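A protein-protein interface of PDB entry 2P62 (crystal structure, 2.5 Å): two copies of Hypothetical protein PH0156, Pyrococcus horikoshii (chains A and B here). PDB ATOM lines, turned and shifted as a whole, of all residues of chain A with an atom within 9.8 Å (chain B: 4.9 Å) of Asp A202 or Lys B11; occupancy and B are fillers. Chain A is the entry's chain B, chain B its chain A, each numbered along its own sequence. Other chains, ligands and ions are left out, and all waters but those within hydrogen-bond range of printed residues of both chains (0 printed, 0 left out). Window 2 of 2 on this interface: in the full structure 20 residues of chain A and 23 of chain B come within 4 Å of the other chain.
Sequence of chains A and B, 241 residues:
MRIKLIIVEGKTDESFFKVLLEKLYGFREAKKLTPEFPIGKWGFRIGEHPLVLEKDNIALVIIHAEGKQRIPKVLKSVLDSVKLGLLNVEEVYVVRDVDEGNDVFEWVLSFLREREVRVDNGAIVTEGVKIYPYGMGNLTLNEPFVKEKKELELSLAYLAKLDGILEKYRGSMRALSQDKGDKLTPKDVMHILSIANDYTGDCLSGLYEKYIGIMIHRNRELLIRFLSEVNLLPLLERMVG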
ATOM      1  N   LYS A  11      14.183   1.713   2.704  1.00  0.00           N
ATOM      2  CA  LYS A  11      15.592   1.296   2.736  1.00  0.00           C
ATOM      3  C   LYS A  11      15.752  -0.158   3.187  1.00  0.00           C
ATOM      4  O   LYS A  11      16.564  -0.908   2.634  1.00  0.00           O
ATOM      5  CB  LYS A  11      16.375   2.221   3.681  1.00  0.00           C
ATOM      6  CG  LYS A  11      17.873   1.978   3.719  1.00  0.00           C
ATOM      7  CD  LYS A  11      18.454   2.088   2.337  1.00  0.00           C
ATOM      8  CE  LYS A  11      19.946   1.883   2.350  1.00  0.00           C
ATOM      9  NZ  LYS A  11      20.508   2.233   1.013  1.00  0.00           N
ATOM     10  N   THR A  12      14.988  -0.549   4.204  1.00  0.00           N
ATOM     11  CA  THR A  12      15.042  -1.912   4.717  1.00  0.00           C
ATOM     12  C   THR A  12      14.734  -2.921   3.607  1.00  0.00           C
ATOM     13  O   THR A  12      15.412  -3.944   3.485  1.00  0.00           O
ATOM     14  CB  THR A  12      14.037  -2.123   5.878  1.00  0.00           C
ATOM     15  OG1 THR A  12      12.776  -1.532   5.536  1.00  0.00           O
ATOM     16  CG2 THR A  12      14.559  -1.493   7.168  1.00  0.00           C
ATOM     17  N   HIS A 191      15.231  -6.313  16.610  1.00  0.00           N
ATOM     18  CA  HIS A 191      16.152  -5.679  17.545  1.00  0.00           C
ATOM     19  C   HIS A 191      16.875  -6.691  18.434  1.00  0.00           C
ATOM     20  O   HIS A 191      17.971  -6.425  18.931  1.00  0.00           O
ATOM     21  CB  HIS A 191      15.431  -4.601  18.353  1.00  0.00           C
ATOM     22  CG  HIS A 191      15.081  -3.395  17.531  1.00  0.00           C
ATOM     23  ND1 HIS A 191      16.039  -2.549  17.008  1.00  0.00           N
ATOM     24  CD2 HIS A 191      13.891  -2.932  17.088  1.00  0.00           C
ATOM     25  CE1 HIS A 191      15.450  -1.620  16.277  1.00  0.00           C
ATOM     26  NE2 HIS A 191      14.147  -1.828  16.308  1.00  0.00           N
ATOM     27  N   SER A 194      19.828  -8.010  16.474  1.00  0.00           N
ATOM     28  CA  SER A 194      20.957  -7.079  16.521  1.00  0.00           C
ATOM     29  C   SER A 194      21.873  -7.434  17.680  1.00  0.00           C
ATOM     30  O   SER A 194      23.098  -7.472  17.542  1.00  0.00           O
ATOM     31  CB  SER A 194      20.460  -5.643  16.697  1.00  0.00           C
ATOM     32  OG  SER A 194      19.627  -5.250  15.615  1.00  0.00           O
ATOM     33  N   ASP A 198      25.578  -9.170  17.746  1.00  0.00           N
ATOM     34  CA  ASP A 198      26.449  -8.095  18.223  1.00  0.00           C
ATOM     35  C   ASP A 198      26.583  -6.997  17.167  1.00  0.00           C
ATOM     36  O   ASP A 198      27.673  -6.462  16.945  1.00  0.00           O
ATOM     37  CB  ASP A 198      27.850  -8.611  18.579  1.00  0.00           C
ATOM     38  CG  ASP A 198      28.620  -7.623  19.454  1.00  0.00           C
ATOM     39  OD1 ASP A 198      29.867  -7.540  19.334  1.00  0.00           O
ATOM     40  OD2 ASP A 198      27.969  -6.934  20.281  1.00  0.00           O
ATOM     41  N   TYR A 199      25.467  -6.668  16.521  1.00  0.00           N
ATOM     42  CA  TYR A 199      25.444  -5.638  15.485  1.00  0.00           C
ATOM     43  C   TYR A 199      25.670  -4.255  16.087  1.00  0.00           C
ATOM     44  O   TYR A 199      24.943  -3.847  16.984  1.00  0.00           O
ATOM     45  CB  TYR A 199      24.100  -5.659  14.761  1.00  0.00           C
ATOM     46  CG  TYR A 199      24.016  -4.683  13.614  1.00  0.00           C
ATOM     47  CD1 TYR A 199      24.867  -4.805  12.510  1.00  0.00           C
ATOM     48  CD2 TYR A 199      23.089  -3.632  13.631  1.00  0.00           C
ATOM     49  CE1 TYR A 199      24.799  -3.908  11.449  1.00  0.00           C
ATOM     50  CE2 TYR A 199      23.011  -2.724  12.580  1.00  0.00           C
ATOM     51  CZ  TYR A 199      23.870  -2.867  11.487  1.00  0.00           C
ATOM     52  OH  TYR A 199      23.805  -1.968  10.441  1.00  0.00           O
ATOM     53  N   THR A 200      26.663  -3.527  15.586  1.00  0.00           N
ATOM     54  CA  THR A 200      26.951  -2.198  16.120  1.00  0.00           C
ATOM     55  C   THR A 200      26.551  -1.060  15.180  1.00  0.00           C
ATOM     56  O   THR A 200      26.830   0.106  15.453  1.00  0.00           O
ATOM     57  CB  THR A 200      28.443  -2.056  16.454  1.00  0.00           C
ATOM     58  OG1 THR A 200      29.202  -2.264  15.262  1.00  0.00           O
ATOM     59  CG2 THR A 200      28.869  -3.093  17.496  1.00  0.00           C
ATOM     60  N   GLY A 201      25.887  -1.402  14.081  1.00  0.00           N
ATOM     61  CA  GLY A 201      25.478  -0.388  13.128  1.00  0.00           C
ATOM     62  C   GLY A 201      24.272   0.411  13.575  1.00  0.00           C
ATOM     63  O   GLY A 201      23.572   0.048  14.523  1.00  0.00           O
ATOM     64  N   ASP A 202      24.031   1.511  12.875  1.00  0.00           N
ATOM     65  CA  ASP A 202      22.915   2.395  13.171  1.00  0.00           C
ATOM     66  C   ASP A 202      21.584   1.904  12.591  1.00  0.00           C
ATOM     67  O   ASP A 202      20.544   2.013  13.240  1.00  0.00           O
ATOM     68  CB  ASP A 202      23.244   3.804  12.639  1.00  0.00           C
ATOM     69  CG  ASP A 202      22.103   4.810  12.826  1.00  0.00           C
ATOM     70  OD1 ASP A 202      21.260   4.653  13.733  1.00  0.00           O
ATOM     71  OD2 ASP A 202      22.068   5.797  12.064  1.00  0.00           O
ATOM     72  N   CYS A 203      21.614   1.337  11.388  1.00  0.00           N
ATOM     73  CA  CYS A 203      20.378   0.901  10.750  1.00  0.00           C
ATOM     74  C   CYS A 203      20.173  -0.604  10.565  1.00  0.00           C
ATOM     75  O   CYS A 203      21.097  -1.340  10.209  1.00  0.00           O
ATOM     76  CB  CYS A 203      20.228   1.610   9.395  1.00  0.00           C
ATOM     77  SG  CYS A 203      20.532   3.411   9.369  1.00  0.00           S
ATOM     78  N   LEU A 204      18.939  -1.045  10.802  1.00  0.00           N
ATOM     79  CA  LEU A 204      18.578  -2.453  10.657  1.00  0.00           C
ATOM     80  C   LEU A 204      18.813  -2.892   9.213  1.00  0.00           C
ATOM     81  O   LEU A 204      19.177  -4.046   8.947  1.00  0.00           O
ATOM     82  CB  LEU A 204      17.109  -2.666  11.044  1.00  0.00           C
ATOM     83  CG  LEU A 204      16.799  -2.357  12.513  1.00  0.00           C
ATOM     84  CD1 LEU A 204      15.300  -2.346  12.761  1.00  0.00           C
ATOM     85  CD2 LEU A 204      17.483  -3.387  13.386  1.00  0.00           C
ATOM     86  N   SER A 205      18.614  -1.968   8.278  1.00  0.00           N
ATOM     87  CA  SER A 205      18.831  -2.294   6.881  1.00  0.00           C
ATOM     88  C   SER A 205      20.275  -2.752   6.699  1.00  0.00           C
ATOM     89  O   SER A 205      20.547  -3.645   5.895  1.00  0.00           O
ATOM     90  CB  SER A 205      18.523  -1.088   5.984  1.00  0.00           C
ATOM     91  OG  SER A 205      19.379   0.005   6.243  1.00  0.00           O
ATOM     92  N   GLY A 206      21.197  -2.164   7.458  1.00  0.00           N
ATOM     93  CA  GLY A 206      22.596  -2.555   7.347  1.00  0.00           C
ATOM     94  C   GLY A 206      22.818  -3.965   7.868  1.00  0.00           C
ATOM     95  O   GLY A 206      23.605  -4.745   7.319  1.00  0.00           O
ATOM     96  N   LEU A 207      22.109  -4.280   8.951  1.00  0.00           N
ATOM     97  CA  LEU A 207      22.170  -5.584   9.591  1.00  0.00           C
ATOM     98  C   LEU A 207      21.728  -6.691   8.645  1.00  0.00           C
ATOM     99  O   LEU A 207      22.295  -7.781   8.653  1.00  0.00           O
ATOM    100  CB  LEU A 207      21.263  -5.613  10.831  1.00  0.00           C
ATOM    101  CG  LEU A 207      21.066  -7.015  11.434  1.00  0.00           C
ATOM    102  CD1 LEU A 207      22.414  -7.520  11.932  1.00  0.00           C
ATOM    103  CD2 LEU A 207      20.026  -6.997  12.575  1.00  0.00           C
ATOM    104  N   TYR A 208      20.702  -6.419   7.845  1.00  0.00           N
ATOM    105  CA  TYR A 208      20.181  -7.425   6.919  1.00  0.00           C
ATOM    106  C   TYR A 208      21.216  -7.781   5.866  1.00  0.00           C
ATOM    107  O   TYR A 208      21.347  -8.950   5.495  1.00  0.00           O
ATOM    108  CB  TYR A 208      18.899  -6.920   6.251  1.00  0.00           C
ATOM    109  CG  TYR A 208      17.826  -6.543   7.248  1.00  0.00           C
ATOM    110  CD1 TYR A 208      16.856  -5.593   6.933  1.00  0.00           C
ATOM    111  CD2 TYR A 208      17.805  -7.104   8.527  1.00  0.00           C
ATOM    112  CE1 TYR A 208      15.903  -5.208   7.870  1.00  0.00           C
ATOM    113  CE2 TYR A 208      16.856  -6.723   9.466  1.00  0.00           C
ATOM    114  CZ  TYR A 208      15.912  -5.778   9.134  1.00  0.00           C
ATOM    115  OH  TYR A 208      14.983  -5.389  10.068  1.00  0.00           O
ATOM    116  N   LYS A 210      24.514  -7.425   6.206  1.00  0.00           N
ATOM    117  CA  LYS A 210      25.605  -8.098   6.898  1.00  0.00           C
ATOM    118  C   LYS A 210      25.242  -9.544   7.206  1.00  0.00           C
ATOM    119  O   LYS A 210      25.973 -10.466   6.851  1.00  0.00           O
ATOM    120  CB  LYS A 210      25.936  -7.360   8.200  1.00  0.00           C
ATOM    121  CG  LYS A 210      27.135  -7.933   8.942  1.00  0.00           C
ATOM    122  CD  LYS A 210      27.349  -7.261  10.287  1.00  0.00           C
ATOM    123  CE  LYS A 210      28.547  -7.866  11.014  1.00  0.00           C
ATOM    124  NZ  LYS A 210      28.822  -7.199  12.323  1.00  0.00           N
ATOM    125  N   GLU B   9      31.524  11.478  14.720  1.00  0.00           N
ATOM    126  CA  GLU B   9      31.873  10.264  13.989  1.00  0.00           C
ATOM    127  C   GLU B   9      30.823   9.736  13.013  1.00  0.00           C
ATOM    128  O   GLU B   9      31.160   9.400  11.883  1.00  0.00           O
ATOM    129  CB  GLU B   9      32.252   9.139  14.956  1.00  0.00           C
ATOM    130  CG  GLU B   9      32.892   7.956  14.242  1.00  0.00           C
ATOM    131  CD  GLU B   9      33.280   6.836  15.185  1.00  0.00           C
ATOM    132  OE1 GLU B   9      33.762   7.139  16.299  1.00  0.00           O
ATOM    133  OE2 GLU B   9      33.118   5.654  14.806  1.00  0.00           O
ATOM    134  N   GLY B  10      29.565   9.655  13.440  1.00  0.00           N
ATOM    135  CA  GLY B  10      28.527   9.137  12.562  1.00  0.00           C
ATOM    136  C   GLY B  10      27.161   9.793  12.675  1.00  0.00           C
ATOM    137  O   GLY B  10      26.985  10.781  13.397  1.00  0.00           O
ATOM    138  N   LYS B  11      26.190   9.234  11.953  1.00  0.00           N
ATOM    139  CA  LYS B  11      24.821   9.748  11.942  1.00  0.00           C
ATOM    140  C   LYS B  11      24.226   9.789  13.348  1.00  0.00           C
ATOM    141  O   LYS B  11      23.565  10.763  13.711  1.00  0.00           O
ATOM    142  CB  LYS B  11      23.933   8.881  11.047  1.00  0.00           C
ATOM    143  CG  LYS B  11      22.639   9.549  10.601  1.00  0.00           C
ATOM    144  CD  LYS B  11      22.924  10.612   9.550  1.00  0.00           C
ATOM    145  CE  LYS B  11      21.656  11.084   8.822  1.00  0.00           C
ATOM    146  NZ  LYS B  11      20.689  11.788   9.705  1.00  0.00           N
ATOM    147  N   THR B  12      24.451   8.737  14.135  1.00  0.00           N
ATOM    148  CA  THR B  12      23.921   8.691  15.497  1.00  0.00           C
ATOM    149  C   THR B  12      24.350   9.925  16.297  1.00  0.00           C
ATOM    150  O   THR B  12      23.526  10.554  16.971  1.00  0.00           O
ATOM    151  CB  THR B  12      24.381   7.413  16.262  1.00  0.00           C
ATOM    152  OG1 THR B  12      25.806   7.272  16.169  1.00  0.00           O
ATOM    153  CG2 THR B  12      23.708   6.164  15.688  1.00  0.00           C
ATOM    154  N   ASP B  13      25.636  10.275  16.210  1.00  0.00           N
ATOM    155  CA  ASP B  13      26.167  11.436  16.924  1.00  0.00           C
ATOM    156  C   ASP B  13      25.596  12.724  16.345  1.00  0.00           C
ATOM    157  O   ASP B  13      25.364  13.684  17.077  1.00  0.00           O
ATOM    158  CB  ASP B  13      27.703  11.483  16.852  1.00  0.00           C
ATOM    159  CG  ASP B  13      28.354  10.114  17.080  1.00  0.00           C
ATOM    160  OD1 ASP B  13      28.778   9.490  16.085  1.00  0.00           O
ATOM    161  OD2 ASP B  13      28.436   9.661  18.243  1.00  0.00           O
ATOM    162  N   GLU B  14      25.364  12.755  15.033  1.00  0.00           N
ATOM    163  CA  GLU B  14      24.806  13.958  14.421  1.00  0.00           C
ATOM    164  C   GLU B  14      23.355  14.196  14.861  1.00  0.00           C
ATOM    165  O   GLU B  14      22.956  15.334  15.099  1.00  0.00           O
ATOM    166  CB  GLU B  14      24.879  13.882  12.888  1.00  0.00           C
ATOM    167  CG  GLU B  14      24.145  15.031  12.181  1.00  0.00           C
ATOM    168  CD  GLU B  14      23.867  14.743  10.710  1.00  0.00           C
ATOM    169  OE1 GLU B  14      24.792  14.856   9.879  1.00  0.00           O
ATOM    170  OE2 GLU B  14      22.717  14.386  10.385  1.00  0.00           O
ATOM    171  N   SER B  15      22.567  13.127  14.967  1.00  0.00           N
ATOM    172  CA  SER B  15      21.169  13.261  15.381  1.00  0.00           C
ATOM    173  C   SER B  15      21.064  13.737  16.816  1.00  0.00           C
ATOM    174  O   SER B  15      20.271  14.627  17.129  1.00  0.00           O
ATOM    175  CB  SER B  15      20.422  11.930  15.255  1.00  0.00           C
ATOM    176  OG  SER B  15      20.228  11.578  13.906  1.00  0.00           O
ATOM    177  N   HIS B  64      29.969  14.532   9.646  1.00  0.00           N
ATOM    178  CA  HIS B  64      30.237  13.199  10.181  1.00  0.00           C
ATOM    179  C   HIS B  64      30.717  12.282   9.058  1.00  0.00           C
ATOM    180  O   HIS B  64      30.735  12.687   7.895  1.00  0.00           O
ATOM    181  CB  HIS B  64      28.983  12.597  10.813  1.00  0.00           C
ATOM    182  CG  HIS B  64      27.936  12.202   9.821  1.00  0.00           C
ATOM    183  ND1 HIS B  64      27.029  13.096   9.295  1.00  0.00           N
ATOM    184  CD2 HIS B  64      27.660  11.006   9.249  1.00  0.00           C
ATOM    185  CE1 HIS B  64      26.239  12.469   8.443  1.00  0.00           C
ATOM    186  NE2 HIS B  64      26.601  11.200   8.397  1.00  0.00           N
ATOM    187  N   ASP B 202      14.020   2.424  10.891  1.00  0.00           N
ATOM    188  CA  ASP B 202      15.168   1.613  10.500  1.00  0.00           C
ATOM    189  C   ASP B 202      16.437   1.937  11.300  1.00  0.00           C
ATOM    190  O   ASP B 202      17.188   1.039  11.700  1.00  0.00           O
ATOM    191  CB  ASP B 202      15.443   1.813   9.005  1.00  0.00           C
ATOM    192  CG  ASP B 202      16.667   1.060   8.526  1.00  0.00           C
ATOM    193  OD1 ASP B 202      16.911  -0.062   9.023  1.00  0.00           O
ATOM    194  OD2 ASP B 202      17.382   1.580   7.640  1.00  0.00           O
ATOM    195  N   CYS B 203      16.671   3.222  11.545  1.00  0.00           N
ATOM    196  CA  CYS B 203      17.875   3.622  12.248  1.00  0.00           C
ATOM    197  C   CYS B 203      17.700   4.095  13.684  1.00  0.00           C
ATOM    198  O   CYS B 203      16.726   4.763  14.037  1.00  0.00           O
ATOM    199  CB  CYS B 203      18.602   4.694  11.436  1.00  0.00           C
ATOM    200  SG  CYS B 203      18.730   4.335   9.651  1.00  0.00           S
ATOM    201  N   LEU B 204      18.667   3.724  14.508  1.00  0.00           N
ATOM    202  CA  LEU B 204      18.661   4.105  15.904  1.00  0.00           C
ATOM    203  C   LEU B 204      18.803   5.622  16.005  1.00  0.00           C
ATOM    204  O   LEU B 204      18.276   6.243  16.928  1.00  0.00           O
ATOM    205  CB  LEU B 204      19.813   3.418  16.636  1.00  0.00           C
ATOM    206  CG  LEU B 204      19.718   1.895  16.764  1.00  0.00           C
ATOM    207  CD1 LEU B 204      21.021   1.374  17.333  1.00  0.00           C
ATOM    208  CD2 LEU B 204      18.534   1.500  17.652  1.00  0.00           C
ATOM    209  N   SER B 205      19.518   6.218  15.052  1.00  0.00           N
ATOM    210  CA  SER B 205      19.707   7.658  15.051  1.00  0.00           C
ATOM    211  C   SER B 205      18.346   8.339  15.047  1.00  0.00           C
ATOM    212  O   SER B 205      18.155   9.359  15.703  1.00  0.00           O
ATOM    213  CB  SER B 205      20.518   8.090  13.826  1.00  0.00           C
ATOM    214  OG  SER B 205      19.865   7.743  12.611  1.00  0.00           O
ATOM    215  N   GLU B 209      16.440  11.089  18.070  1.00  0.00           N
ATOM    216  CA  GLU B 209      15.738  12.338  17.753  1.00  0.00           C
ATOM    217  C   GLU B 209      14.319  12.290  18.306  1.00  0.00           C
ATOM    218  O   GLU B 209      13.868  13.220  18.973  1.00  0.00           O
ATOM    219  CB  GLU B 209      15.655  12.560  16.231  1.00  0.00           C
ATOM    220  CG  GLU B 209      16.968  12.961  15.560  1.00  0.00           C
ATOM    221  CD  GLU B 209      16.837  13.190  14.052  1.00  0.00           C
ATOM    222  OE1 GLU B 209      16.021  14.046  13.643  1.00  0.00           O
ATOM    223  OE2 GLU B 209      17.553  12.509  13.282  1.00  0.00           O
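Of chain A, only Asp A202 (3.7 Å) comes within 4 Å of Lys B11.
Thr B12 touches just one residue of chain A: Asp A202 (3.5 Å).
No residue of chain A comes within 4 Å of Glu B14.
Of chain A, only Asp A202 and Cys A203 come within 4 Å of Cys B203.
Of the printed residues of chain A, Asp B202 touches Lys A11 (3.97 Å), Thr A12 (3.3 Å), Asp A202 (3.8 Å), Cys A203 (3.3 Å), Leu A204 (2.9 Å) and Ser A205 (2.7 Å).
Printed residues of chain B within 4 Å of Thr A12: Asp B202.
Of the printed residues of chain A, Ser B205 touches Asp A202 (2.7 Å).
Of the printed residues of chain B, Lys A11 touches Asp B202.
Asp A198 touches none of the printed residues of chain B.
The nearest printed residue of chain B that does not touch Asp A202 is Ser B15 (6.3 Å).
The nearest residue of chain A that does not touch Lys B11 is Cys A203 (6.6 Å).
Printed residues of chain B that touch a printed residue of chain A: Lys B11, Thr B12, Asp B202, Cys B203, Leu B204 and Ser B205.
Of the 16 printed residues of chain A, 6 touch a printed residue of chain B.
Hydrophobic or aromatic side chains of chain A that line the printed part of chain B: Leu A204.
Among the printed residues, no Asp or Glu carboxylate lies within 4 Å of a Lys or Arg side-chain nitrogen of the other chain.
The backbone carbonyl oxygen (O) of Asp A202 sits at hydrogen-bond distance from the backbone NH (N) of Leu B204, at 2.8 Å.
The side-chain carboxylate (OD1) of Asp B202 is in hydrogen-bond range of the backbone NH (N) of Ser A205, at 2.7 Å.
The backbone NH (N) of Leu A204 is in hydrogen-bond range of the backbone carbonyl oxygen (O) of Asp B202 (2.9 Å).
The side-chain sulfur of Cys A203 is disulfide-bonded to the side-chain sulfur of Cys B203, 2.0 Å away.
N of Ser B205 lies within hydrogen-bond range of OD1 of Asp A202 (2.7 Å).
OE2 of Glu B14 is in salt-bridge range of NZ of Lys B11 (3.4 Å).
The side-chain hydroxyl (OG) of Ser B15 sits at hydrogen-bond distance from the backbone carbonyl oxygen (O) of Lys B11 (3.4 Å).
The backbone carbonyl oxygen (O) of Cys A203 sits at hydrogen-bond distance from the side-chain hydroxyl (OH) of Tyr A199 (2.8 Å).
Among the printed residues, merely in contact across the chains: Lys A11 with Asp B202, Thr A12 with Asp B202, Asp A202 with Lys B11, Asp A202 with Thr B12, Asp A202 with Asp B202, Asp A202 with Cys B203 and Cys A203 with Asp B202.
Thr A12 touches Asp B202, and with the chains exchanged Asp A202 touches Thr B12.
Asp A202 touches its own counterpart, Asp B202.
Asp A202 touches Ser B205, and with the chains exchanged Ser A205 touches Asp B202.
Cys B203 touches its own counterpart, Cys A203.
Positions printed for both chains: 11, 12, 202, 203, 204 and 205.
Of the 12 pairs that touch across the chains among the printed residues, 12 have their exchanged pair printed and touching as well.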
